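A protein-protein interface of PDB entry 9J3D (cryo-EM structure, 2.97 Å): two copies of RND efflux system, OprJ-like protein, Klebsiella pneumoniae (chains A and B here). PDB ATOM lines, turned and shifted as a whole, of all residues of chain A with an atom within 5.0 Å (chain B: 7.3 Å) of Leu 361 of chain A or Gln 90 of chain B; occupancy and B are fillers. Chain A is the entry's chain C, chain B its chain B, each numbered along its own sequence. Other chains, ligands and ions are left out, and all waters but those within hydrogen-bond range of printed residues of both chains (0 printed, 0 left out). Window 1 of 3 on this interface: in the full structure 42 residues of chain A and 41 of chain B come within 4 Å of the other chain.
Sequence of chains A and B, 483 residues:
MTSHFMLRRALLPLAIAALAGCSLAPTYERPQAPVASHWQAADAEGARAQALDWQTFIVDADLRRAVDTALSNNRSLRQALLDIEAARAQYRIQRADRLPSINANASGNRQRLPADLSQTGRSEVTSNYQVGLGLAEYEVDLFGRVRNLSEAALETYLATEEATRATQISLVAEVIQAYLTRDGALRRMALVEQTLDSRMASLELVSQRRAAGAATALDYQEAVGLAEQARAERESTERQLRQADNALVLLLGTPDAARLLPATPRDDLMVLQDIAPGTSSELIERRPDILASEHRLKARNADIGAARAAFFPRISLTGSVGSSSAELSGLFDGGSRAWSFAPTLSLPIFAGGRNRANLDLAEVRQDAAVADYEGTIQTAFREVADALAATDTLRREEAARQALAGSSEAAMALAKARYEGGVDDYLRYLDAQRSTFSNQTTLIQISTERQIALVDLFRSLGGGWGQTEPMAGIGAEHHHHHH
Of the 11 printed residues of chain A, 4 touch a printed residue of chain B. Hydrophobic or aromatic side chains of chain A that line the printed part of chain B: Ala 357, Leu 361 and Val 364. Along chain A the printed residues that touch a printed residue of chain B span positions 357 to 364. Printed residues of chain B that touch a printed residue of chain A: Glu 85, Ala 86, Ala 89, Gln 90 and Ile 93. Hydrophobic or aromatic side chains of chain B within 4 Å of the printed part of chain A: Ala 86, Ala 89 and Ile 93. Among the printed residues, no Asp or Glu carboxylate lies within 4 Å of a Lys or Arg side-chain nitrogen of the other chain.
CB of Ala 357 of chain A touches O of Ala 89 of chain B, 3.5 Å away. CB of Ala 357 of chain A touches CG1 of Ile 93 of chain B, 3.4 Å away. CD1 of Ile 93 of chain B touches OD1 of Asn 358 of chain A, 3.2 Å away. Leu 361 of chain A touches Ala 89 of chain B. Leu 361 of chain A touches Gln 90 of chain B (CD2 to NE2, 3.5 Å). Val 364 of chain A touches Glu 85 of chain B (CG2 to OE1, 3.6 Å). Ala 86 of chain B touches Val 364 of chain A.
No position is printed for both chains. Of the 7 pairs that touch across the chains among the printed residues, none has its exchanged pair printed and touching as well.
The guanidinium group (NH2) of Arg 88 of chain B is in hydrogen-bond range of the backbone carbonyl oxygen (O) of Glu 85 of chain B, at 2.9 Å. NE2 of Gln 90 of chain B lies close to O of Ala 86 of chain B, 3.1 Å away.
Printed residues of chain B within 4 Å of Leu 361 of chain A: Ala 89 (3.9 Å) and Gln 90 (3.5 Å). Gln 90 of chain B touches just one residue of chain A: Leu 361. Printed residues of chain B within 4 Å of Ala 357 of chain A: Ala 89 and Ile 93. Printed residues of chain B within 4 Å of Val 364 of chain A: Glu 85 (3.6 Å) and Ala 86 (3.5 Å). Gln 94 of chain B touches none of the printed residues of chain A. Thr 156 of chain B touches none of the printed residues of chain A. The nearest printed residue of chain B that does not touch Ala 357 of chain A is Arg 92 of chain B (4.04 Å).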
ATOM      1  N   ARG A 300      -2.671   7.365  19.208  1.00  0.00           N
ATOM      2  CA  ARG A 300      -3.120   8.646  18.675  1.00  0.00           C
ATOM      3  C   ARG A 300      -2.073   9.264  17.755  1.00  0.00           C
ATOM      4  O   ARG A 300      -2.411   9.796  16.688  1.00  0.00           O
ATOM      5  CB  ARG A 300      -3.439   9.596  19.826  1.00  0.00           C
ATOM      6  CG  ARG A 300      -4.874   9.542  20.301  1.00  0.00           C
ATOM      7  CD  ARG A 300      -5.808  10.181  19.299  1.00  0.00           C
ATOM      8  NE  ARG A 300      -5.220  11.365  18.684  1.00  0.00           N
ATOM      9  CZ  ARG A 300      -4.852  11.443  17.414  1.00  0.00           C
ATOM     10  NH1 ARG A 300      -5.008  10.426  16.588  1.00  0.00           N
ATOM     11  NH2 ARG A 300      -4.323  12.574  16.958  1.00  0.00           N
ATOM     12  N   ALA A 357      -9.646  19.302   7.162  1.00  0.00           N
ATOM     13  CA  ALA A 357     -10.311  19.218   8.457  1.00  0.00           C
ATOM     14  C   ALA A 357     -10.084  17.859   9.107  1.00  0.00           C
ATOM     15  O   ALA A 357     -10.103  17.743  10.336  1.00  0.00           O
ATOM     16  CB  ALA A 357     -11.800  19.522   8.312  1.00  0.00           C
ATOM     17  N   ASN A 358      -9.824  16.825   8.303  1.00  0.00           N
ATOM     18  CA  ASN A 358      -9.322  15.573   8.862  1.00  0.00           C
ATOM     19  C   ASN A 358      -7.991  15.789   9.570  1.00  0.00           C
ATOM     20  O   ASN A 358      -7.751  15.230  10.648  1.00  0.00           O
ATOM     21  CB  ASN A 358      -9.173  14.525   7.758  1.00  0.00           C
ATOM     22  CG  ASN A 358     -10.433  13.708   7.548  1.00  0.00           C
ATOM     23  OD1 ASN A 358     -11.279  13.613   8.434  1.00  0.00           O
ATOM     24  ND2 ASN A 358     -10.561  13.112   6.367  1.00  0.00           N
ATOM     25  N   LEU A 359      -7.116  16.602   8.976  1.00  0.00           N
ATOM     26  CA  LEU A 359      -5.822  16.891   9.584  1.00  0.00           C
ATOM     27  C   LEU A 359      -5.991  17.647  10.900  1.00  0.00           C
ATOM     28  O   LEU A 359      -5.323  17.339  11.896  1.00  0.00           O
ATOM     29  CB  LEU A 359      -4.963  17.684   8.595  1.00  0.00           C
ATOM     30  CG  LEU A 359      -3.436  17.721   8.673  1.00  0.00           C
ATOM     31  CD1 LEU A 359      -2.924  18.639   9.771  1.00  0.00           C
ATOM     32  CD2 LEU A 359      -2.917  16.317   8.861  1.00  0.00           C
ATOM     33  N   ASP A 360      -6.886  18.640  10.923  1.00  0.00           N
ATOM     34  CA  ASP A 360      -7.162  19.339  12.178  1.00  0.00           C
ATOM     35  C   ASP A 360      -7.760  18.400  13.215  1.00  0.00           C
ATOM     36  O   ASP A 360      -7.436  18.493  14.404  1.00  0.00           O
ATOM     37  CB  ASP A 360      -8.085  20.539  11.952  1.00  0.00           C
ATOM     38  CG  ASP A 360      -7.637  21.422  10.808  1.00  0.00           C
ATOM     39  OD1 ASP A 360      -7.444  20.907   9.698  1.00  0.00           O
ATOM     40  OD2 ASP A 360      -7.482  22.642  11.014  1.00  0.00           O
ATOM     41  N   LEU A 361      -8.639  17.492  12.787  1.00  0.00           N
ATOM     42  CA  LEU A 361      -9.199  16.513  13.710  1.00  0.00           C
ATOM     43  C   LEU A 361      -8.099  15.666  14.333  1.00  0.00           C
ATOM     44  O   LEU A 361      -8.087  15.449  15.550  1.00  0.00           O
ATOM     45  CB  LEU A 361     -10.230  15.651  12.972  1.00  0.00           C
ATOM     46  CG  LEU A 361     -10.934  14.417  13.557  1.00  0.00           C
ATOM     47  CD1 LEU A 361     -10.035  13.189  13.640  1.00  0.00           C
ATOM     48  CD2 LEU A 361     -11.527  14.742  14.921  1.00  0.00           C
ATOM     49  N   ALA A 362      -7.153  15.201  13.517  1.00  0.00           N
ATOM     50  CA  ALA A 362      -6.052  14.398  14.042  1.00  0.00           C
ATOM     51  C   ALA A 362      -5.186  15.195  15.011  1.00  0.00           C
ATOM     52  O   ALA A 362      -4.832  14.698  16.088  1.00  0.00           O
ATOM     53  CB  ALA A 362      -5.203  13.854  12.895  1.00  0.00           C
ATOM     54  N   GLU A 363      -4.832  16.430  14.648  1.00  0.00           N
ATOM     55  CA  GLU A 363      -3.980  17.239  15.518  1.00  0.00           C
ATOM     56  C   GLU A 363      -4.666  17.524  16.850  1.00  0.00           C
ATOM     57  O   GLU A 363      -4.047  17.443  17.920  1.00  0.00           O
ATOM     58  CB  GLU A 363      -3.606  18.546  14.821  1.00  0.00           C
ATOM     59  CG  GLU A 363      -2.558  18.409  13.735  1.00  0.00           C
ATOM     60  CD  GLU A 363      -2.272  19.726  13.042  1.00  0.00           C
ATOM     61  OE1 GLU A 363      -3.045  20.685  13.246  1.00  0.00           O
ATOM     62  OE2 GLU A 363      -1.273  19.806  12.298  1.00  0.00           O
ATOM     63  N   VAL A 364      -5.953  17.862  16.801  1.00  0.00           N
ATOM     64  CA  VAL A 364      -6.687  18.175  18.019  1.00  0.00           C
ATOM     65  C   VAL A 364      -6.845  16.931  18.882  1.00  0.00           C
ATOM     66  O   VAL A 364      -6.749  16.993  20.116  1.00  0.00           O
ATOM     67  CB  VAL A 364      -8.043  18.805  17.662  1.00  0.00           C
ATOM     68  CG1 VAL A 364      -8.902  18.877  18.875  1.00  0.00           C
ATOM     69  CG2 VAL A 364      -7.840  20.194  17.077  1.00  0.00           C
ATOM     70  N   ARG A 365      -7.091  15.780  18.252  1.00  0.00           N
ATOM     71  CA  ARG A 365      -7.143  14.533  19.000  1.00  0.00           C
ATOM     72  C   ARG A 365      -5.809  14.236  19.673  1.00  0.00           C
ATOM     73  O   ARG A 365      -5.784  13.734  20.800  1.00  0.00           O
ATOM     74  CB  ARG A 365      -7.543  13.389  18.070  1.00  0.00           C
ATOM     75  CG  ARG A 365      -9.038  13.227  17.859  1.00  0.00           C
ATOM     76  CD  ARG A 365      -9.544  11.926  18.472  1.00  0.00           C
ATOM     77  NE  ARG A 365      -8.764  10.758  18.073  1.00  0.00           N
ATOM     78  CZ  ARG A 365      -8.627  10.315  16.829  1.00  0.00           C
ATOM     79  NH1 ARG A 365      -9.255  10.885  15.815  1.00  0.00           N
ATOM     80  NH2 ARG A 365      -7.848   9.262  16.600  1.00  0.00           N
ATOM     81  N   GLN A 366      -4.695  14.545  19.005  1.00  0.00           N
ATOM     82  CA  GLN A 366      -3.386  14.368  19.632  1.00  0.00           C
ATOM     83  C   GLN A 366      -3.217  15.287  20.833  1.00  0.00           C
ATOM     84  O   GLN A 366      -2.655  14.885  21.861  1.00  0.00           O
ATOM     85  CB  GLN A 366      -2.277  14.634  18.623  1.00  0.00           C
ATOM     86  CG  GLN A 366      -0.893  14.726  19.249  1.00  0.00           C
ATOM     87  CD  GLN A 366      -0.327  16.130  19.209  1.00  0.00           C
ATOM     88  OE1 GLN A 366      -0.692  16.936  18.351  1.00  0.00           O
ATOM     89  NE2 GLN A 366       0.576  16.431  20.134  1.00  0.00           N
ATOM     90  N   ASP B  83     -11.605  19.643  22.766  1.00  0.00           N
ATOM     91  CA  ASP B  83     -12.776  18.976  22.210  1.00  0.00           C
ATOM     92  C   ASP B  83     -13.661  19.963  21.465  1.00  0.00           C
ATOM     93  O   ASP B  83     -14.327  19.590  20.494  1.00  0.00           O
ATOM     94  CB  ASP B  83     -13.566  18.275  23.315  1.00  0.00           C
ATOM     95  CG  ASP B  83     -12.882  17.016  23.808  1.00  0.00           C
ATOM     96  OD1 ASP B  83     -12.199  16.354  22.999  1.00  0.00           O
ATOM     97  OD2 ASP B  83     -13.027  16.687  25.004  1.00  0.00           O
ATOM     98  N   ILE B  84     -13.674  21.223  21.903  1.00  0.00           N
ATOM     99  CA  ILE B  84     -14.355  22.263  21.133  1.00  0.00           C
ATOM    100  C   ILE B  84     -13.759  22.357  19.733  1.00  0.00           C
ATOM    101  O   ILE B  84     -14.483  22.390  18.729  1.00  0.00           O
ATOM    102  CB  ILE B  84     -14.281  23.617  21.861  1.00  0.00           C
ATOM    103  CG1 ILE B  84     -15.286  23.673  23.010  1.00  0.00           C
ATOM    104  CG2 ILE B  84     -14.520  24.763  20.891  1.00  0.00           C
ATOM    105  CD1 ILE B  84     -15.332  25.023  23.692  1.00  0.00           C
ATOM    106  N   GLU B  85     -12.428  22.388  19.645  1.00  0.00           N
ATOM    107  CA  GLU B  85     -11.770  22.465  18.343  1.00  0.00           C
ATOM    108  C   GLU B  85     -12.028  21.211  17.517  1.00  0.00           C
ATOM    109  O   GLU B  85     -12.169  21.280  16.293  1.00  0.00           O
ATOM    110  CB  GLU B  85     -10.270  22.687  18.525  1.00  0.00           C
ATOM    111  CG  GLU B  85      -9.906  24.049  19.090  1.00  0.00           C
ATOM    112  CD  GLU B  85      -8.407  24.263  19.166  1.00  0.00           C
ATOM    113  OE1 GLU B  85      -7.655  23.394  18.675  1.00  0.00           O
ATOM    114  OE2 GLU B  85      -7.978  25.298  19.716  1.00  0.00           O
ATOM    115  N   ALA B  86     -12.075  20.050  18.172  1.00  0.00           N
ATOM    116  CA  ALA B  86     -12.349  18.803  17.464  1.00  0.00           C
ATOM    117  C   ALA B  86     -13.752  18.810  16.872  1.00  0.00           C
ATOM    118  O   ALA B  86     -13.959  18.411  15.720  1.00  0.00           O
ATOM    119  CB  ALA B  86     -12.172  17.613  18.405  1.00  0.00           C
ATOM    120  N   ALA B  87     -14.734  19.256  17.656  1.00  0.00           N
ATOM    121  CA  ALA B  87     -16.095  19.361  17.150  1.00  0.00           C
ATOM    122  C   ALA B  87     -16.178  20.377  16.021  1.00  0.00           C
ATOM    123  O   ALA B  87     -16.911  20.176  15.048  1.00  0.00           O
ATOM    124  CB  ALA B  87     -17.047  19.730  18.284  1.00  0.00           C
ATOM    125  N   ARG B  88     -15.425  21.474  16.130  1.00  0.00           N
ATOM    126  CA  ARG B  88     -15.367  22.445  15.042  1.00  0.00           C
ATOM    127  C   ARG B  88     -14.790  21.815  13.780  1.00  0.00           C
ATOM    128  O   ARG B  88     -15.277  22.063  12.672  1.00  0.00           O
ATOM    129  CB  ARG B  88     -14.540  23.657  15.484  1.00  0.00           C
ATOM    130  CG  ARG B  88     -14.425  24.808  14.480  1.00  0.00           C
ATOM    131  CD  ARG B  88     -13.289  24.632  13.468  1.00  0.00           C
ATOM    132  NE  ARG B  88     -12.202  23.785  13.952  1.00  0.00           N
ATOM    133  CZ  ARG B  88     -11.332  24.130  14.893  1.00  0.00           C
ATOM    134  NH1 ARG B  88     -11.380  25.313  15.481  1.00  0.00           N
ATOM    135  NH2 ARG B  88     -10.387  23.264  15.250  1.00  0.00           N
ATOM    136  N   ALA B  89     -13.745  21.001  13.931  1.00  0.00           N
ATOM    137  CA  ALA B  89     -13.141  20.337  12.782  1.00  0.00           C
ATOM    138  C   ALA B  89     -14.109  19.354  12.137  1.00  0.00           C
ATOM    139  O   ALA B  89     -14.187  19.267  10.909  1.00  0.00           O
ATOM    140  CB  ALA B  89     -11.854  19.629  13.201  1.00  0.00           C
ATOM    141  N   GLN B  90     -14.850  18.599  12.950  1.00  0.00           N
ATOM    142  CA  GLN B  90     -15.845  17.683  12.397  1.00  0.00           C
ATOM    143  C   GLN B  90     -16.968  18.444  11.701  1.00  0.00           C
ATOM    144  O   GLN B  90     -17.480  18.005  10.661  1.00  0.00           O
ATOM    145  CB  GLN B  90     -16.405  16.782  13.497  1.00  0.00           C
ATOM    146  CG  GLN B  90     -15.350  15.963  14.226  1.00  0.00           C
ATOM    147  CD  GLN B  90     -15.584  15.908  15.724  1.00  0.00           C
ATOM    148  OE1 GLN B  90     -16.661  16.253  16.209  1.00  0.00           O
ATOM    149  NE2 GLN B  90     -14.570  15.481  16.466  1.00  0.00           N
ATOM    150  N   TYR B  91     -17.369  19.586  12.263  1.00  0.00           N
ATOM    151  CA  TYR B  91     -18.367  20.423  11.608  1.00  0.00           C
ATOM    152  C   TYR B  91     -17.859  20.927  10.266  1.00  0.00           C
ATOM    153  O   TYR B  91     -18.607  20.958   9.284  1.00  0.00           O
ATOM    154  CB  TYR B  91     -18.750  21.589  12.521  1.00  0.00           C
ATOM    155  CG  TYR B  91     -18.945  22.904  11.801  1.00  0.00           C
ATOM    156  CD1 TYR B  91     -17.944  23.868  11.792  1.00  0.00           C
ATOM    157  CD2 TYR B  91     -20.129  23.183  11.135  1.00  0.00           C
ATOM    158  CE1 TYR B  91     -18.117  25.071  11.137  1.00  0.00           C
ATOM    159  CE2 TYR B  91     -20.311  24.382  10.475  1.00  0.00           C
ATOM    160  CZ  TYR B  91     -19.303  25.323  10.479  1.00  0.00           C
ATOM    161  OH  TYR B  91     -19.482  26.521   9.824  1.00  0.00           O
ATOM    162  N   ARG B  92     -16.587  21.322  10.204  1.00  0.00           N
ATOM    163  CA  ARG B  92     -15.999  21.729   8.932  1.00  0.00           C
ATOM    164  C   ARG B  92     -15.952  20.562   7.953  1.00  0.00           C
ATOM    165  O   ARG B  92     -16.179  20.742   6.751  1.00  0.00           O
ATOM    166  CB  ARG B  92     -14.604  22.308   9.157  1.00  0.00           C
ATOM    167  CG  ARG B  92     -14.594  23.604   9.957  1.00  0.00           C
ATOM    168  CD  ARG B  92     -14.648  24.827   9.051  1.00  0.00           C
ATOM    169  NE  ARG B  92     -14.500  26.069   9.803  1.00  0.00           N
ATOM    170  CZ  ARG B  92     -14.161  27.234   9.269  1.00  0.00           C
ATOM    171  NH1 ARG B  92     -13.923  27.358   7.974  1.00  0.00           N
ATOM    172  NH2 ARG B  92     -14.059  28.302  10.054  1.00  0.00           N
ATOM    173  N   ILE B  93     -15.662  19.357   8.452  1.00  0.00           N
ATOM    174  CA  ILE B  93     -15.705  18.161   7.611  1.00  0.00           C
ATOM    175  C   ILE B  93     -17.074  18.021   6.966  1.00  0.00           C
ATOM    176  O   ILE B  93     -17.199  17.893   5.742  1.00  0.00           O
ATOM    177  CB  ILE B  93     -15.372  16.904   8.438  1.00  0.00           C
ATOM    178  CG1 ILE B  93     -13.897  16.857   8.824  1.00  0.00           C
ATOM    179  CG2 ILE B  93     -15.787  15.644   7.686  1.00  0.00           C
ATOM    180  CD1 ILE B  93     -13.027  16.166   7.807  1.00  0.00           C
ATOM    181  N   GLN B  94     -18.124  18.067   7.785  1.00  0.00           N
ATOM    182  CA  GLN B  94     -19.460  17.779   7.276  1.00  0.00           C
ATOM    183  C   GLN B  94     -19.967  18.927   6.409  1.00  0.00           C
ATOM    184  O   GLN B  94     -20.781  18.718   5.502  1.00  0.00           O
ATOM    185  CB  GLN B  94     -20.411  17.508   8.442  1.00  0.00           C
ATOM    186  CG  GLN B  94     -20.434  16.048   8.939  1.00  0.00           C
ATOM    187  CD  GLN B  94     -20.436  14.975   7.849  1.00  0.00           C
ATOM    188  OE1 GLN B  94     -21.481  14.458   7.473  1.00  0.00           O
ATOM    189  NE2 GLN B  94     -19.258  14.632   7.350  1.00  0.00           N
ATOM    190  N   ARG B  95     -19.484  20.147   6.666  1.00  0.00           N
ATOM    191  CA  ARG B  95     -19.884  21.301   5.867  1.00  0.00           C
ATOM    192  C   ARG B  95     -19.186  21.324   4.513  1.00  0.00           C
ATOM    193  O   ARG B  95     -19.782  21.756   3.520  1.00  0.00           O
ATOM    194  CB  ARG B  95     -19.591  22.590   6.635  1.00  0.00           C
ATOM    195  CG  ARG B  95     -20.052  23.863   5.941  1.00  0.00           C
ATOM    196  CD  ARG B  95     -19.732  25.097   6.776  1.00  0.00           C
ATOM    197  NE  ARG B  95     -19.985  26.334   6.046  1.00  0.00           N
ATOM    198  CZ  ARG B  95     -19.579  27.535   6.439  1.00  0.00           C
ATOM    199  NH1 ARG B  95     -18.895  27.700   7.560  1.00  0.00           N
ATOM    200  NH2 ARG B  95     -19.870  28.595   5.691  1.00  0.00           N
ATOM    201  N   ALA B  96     -17.930  20.871   4.451  1.00  0.00           N
ATOM    202  CA  ALA B  96     -17.210  20.867   3.182  1.00  0.00           C
ATOM    203  C   ALA B  96     -17.846  19.914   2.180  1.00  0.00           C
ATOM    204  O   ALA B  96     -17.644  20.062   0.969  1.00  0.00           O
ATOM    205  CB  ALA B  96     -15.746  20.497   3.413  1.00  0.00           C
ATOM    206  N   LEU B 149     -26.749  16.944   7.539  1.00  0.00           N
ATOM    207  CA  LEU B 149     -25.614  16.423   8.298  1.00  0.00           C
ATOM    208  C   LEU B 149     -24.666  17.536   8.729  1.00  0.00           C
ATOM    209  O   LEU B 149     -24.097  17.481   9.827  1.00  0.00           O
ATOM    210  CB  LEU B 149     -24.891  15.332   7.500  1.00  0.00           C
ATOM    211  CG  LEU B 149     -24.278  15.599   6.120  1.00  0.00           C
ATOM    212  CD1 LEU B 149     -22.984  16.400   6.116  1.00  0.00           C
ATOM    213  CD2 LEU B 149     -24.078  14.259   5.397  1.00  0.00           C
ATOM    214  N   SER B 150     -24.491  18.560   7.892  1.00  0.00           N
ATOM    215  CA  SER B 150     -23.690  19.705   8.310  1.00  0.00           C
ATOM    216  C   SER B 150     -24.332  20.416   9.495  1.00  0.00           C
ATOM    217  O   SER B 150     -23.640  20.823  10.435  1.00  0.00           O
ATOM    218  CB  SER B 150     -23.502  20.670   7.141  1.00  0.00           C
ATOM    219  OG  SER B 150     -22.778  21.820   7.543  1.00  0.00           O
ATOM    220  N   ALA B 153     -23.743  18.332  12.593  1.00  0.00           N
ATOM    221  CA  ALA B 153     -22.388  18.551  13.087  1.00  0.00           C
ATOM    222  C   ALA B 153     -22.253  19.902  13.777  1.00  0.00           C
ATOM    223  O   ALA B 153     -21.561  20.011  14.794  1.00  0.00           O
ATOM    224  CB  ALA B 153     -21.387  18.434  11.939  1.00  0.00           C
ATOM    225  N   LEU B 154     -22.895  20.938  13.238  1.00  0.00           N
ATOM    226  CA  LEU B 154     -22.855  22.253  13.874  1.00  0.00           C
ATOM    227  C   LEU B 154     -23.511  22.216  15.250  1.00  0.00           C
ATOM    228  O   LEU B 154     -23.002  22.803  16.213  1.00  0.00           O
ATOM    229  CB  LEU B 154     -23.538  23.281  12.973  1.00  0.00           C
ATOM    230  CG  LEU B 154     -23.679  24.699  13.525  1.00  0.00           C
ATOM    231  CD1 LEU B 154     -22.312  25.300  13.807  1.00  0.00           C
ATOM    232  CD2 LEU B 154     -24.463  25.569  12.556  1.00  0.00           C
ATOM    233  N   THR B 156     -23.774  19.574  17.129  1.00  0.00           N
ATOM    234  CA  THR B 156     -22.853  18.822  17.975  1.00  0.00           C
ATOM    235  C   THR B 156     -21.724  19.711  18.479  1.00  0.00           C
ATOM    236  O   THR B 156     -21.321  19.616  19.643  1.00  0.00           O
ATOM    237  CB  THR B 156     -22.293  17.626  17.205  1.00  0.00           C
ATOM    238  OG1 THR B 156     -23.371  16.794  16.760  1.00  0.00           O
ATOM    239  CG2 THR B 156     -21.361  16.808  18.084  1.00  0.00           C
ATOM    240  N   TYR B 157     -21.199  20.578  17.615  1.00  0.00           N
ATOM    241  CA  TYR B 157     -20.138  21.491  18.031  1.00  0.00           C
ATOM    242  C   TYR B 157     -20.638  22.476  19.083  1.00  0.00           C
ATOM    243  O   TYR B 157     -19.930  22.779  20.053  1.00  0.00           O
ATOM    244  CB  TYR B 157     -19.578  22.222  16.810  1.00  0.00           C
ATOM    245  CG  TYR B 157     -19.142  23.649  17.061  1.00  0.00           C
ATOM    246  CD1 TYR B 157     -17.840  23.940  17.447  1.00  0.00           C
ATOM    247  CD2 TYR B 157     -20.025  24.705  16.891  1.00  0.00           C
ATOM    248  CE1 TYR B 157     -17.438  25.243  17.670  1.00  0.00           C
ATOM    249  CE2 TYR B 157     -19.633  26.007  17.117  1.00  0.00           C
ATOM    250  CZ  TYR B 157     -18.339  26.271  17.504  1.00  0.00           C
ATOM    251  OH  TYR B 157     -17.947  27.571  17.725  1.00  0.00           O
ATOM    252  N   THR B 160     -20.849  20.663  22.274  1.00  0.00           N
ATOM    253  CA  THR B 160     -19.509  20.506  22.823  1.00  0.00           C
ATOM    254  C   THR B 160     -19.032  21.780  23.508  1.00  0.00           C
ATOM    255  O   THR B 160     -18.417  21.714  24.577  1.00  0.00           O
ATOM    256  CB  THR B 160     -18.535  20.101  21.718  1.00  0.00           C
ATOM    257  OG1 THR B 160     -18.949  18.854  21.149  1.00  0.00           O
ATOM    258  CG2 THR B 160     -17.126  19.954  22.271  1.00  0.00           C
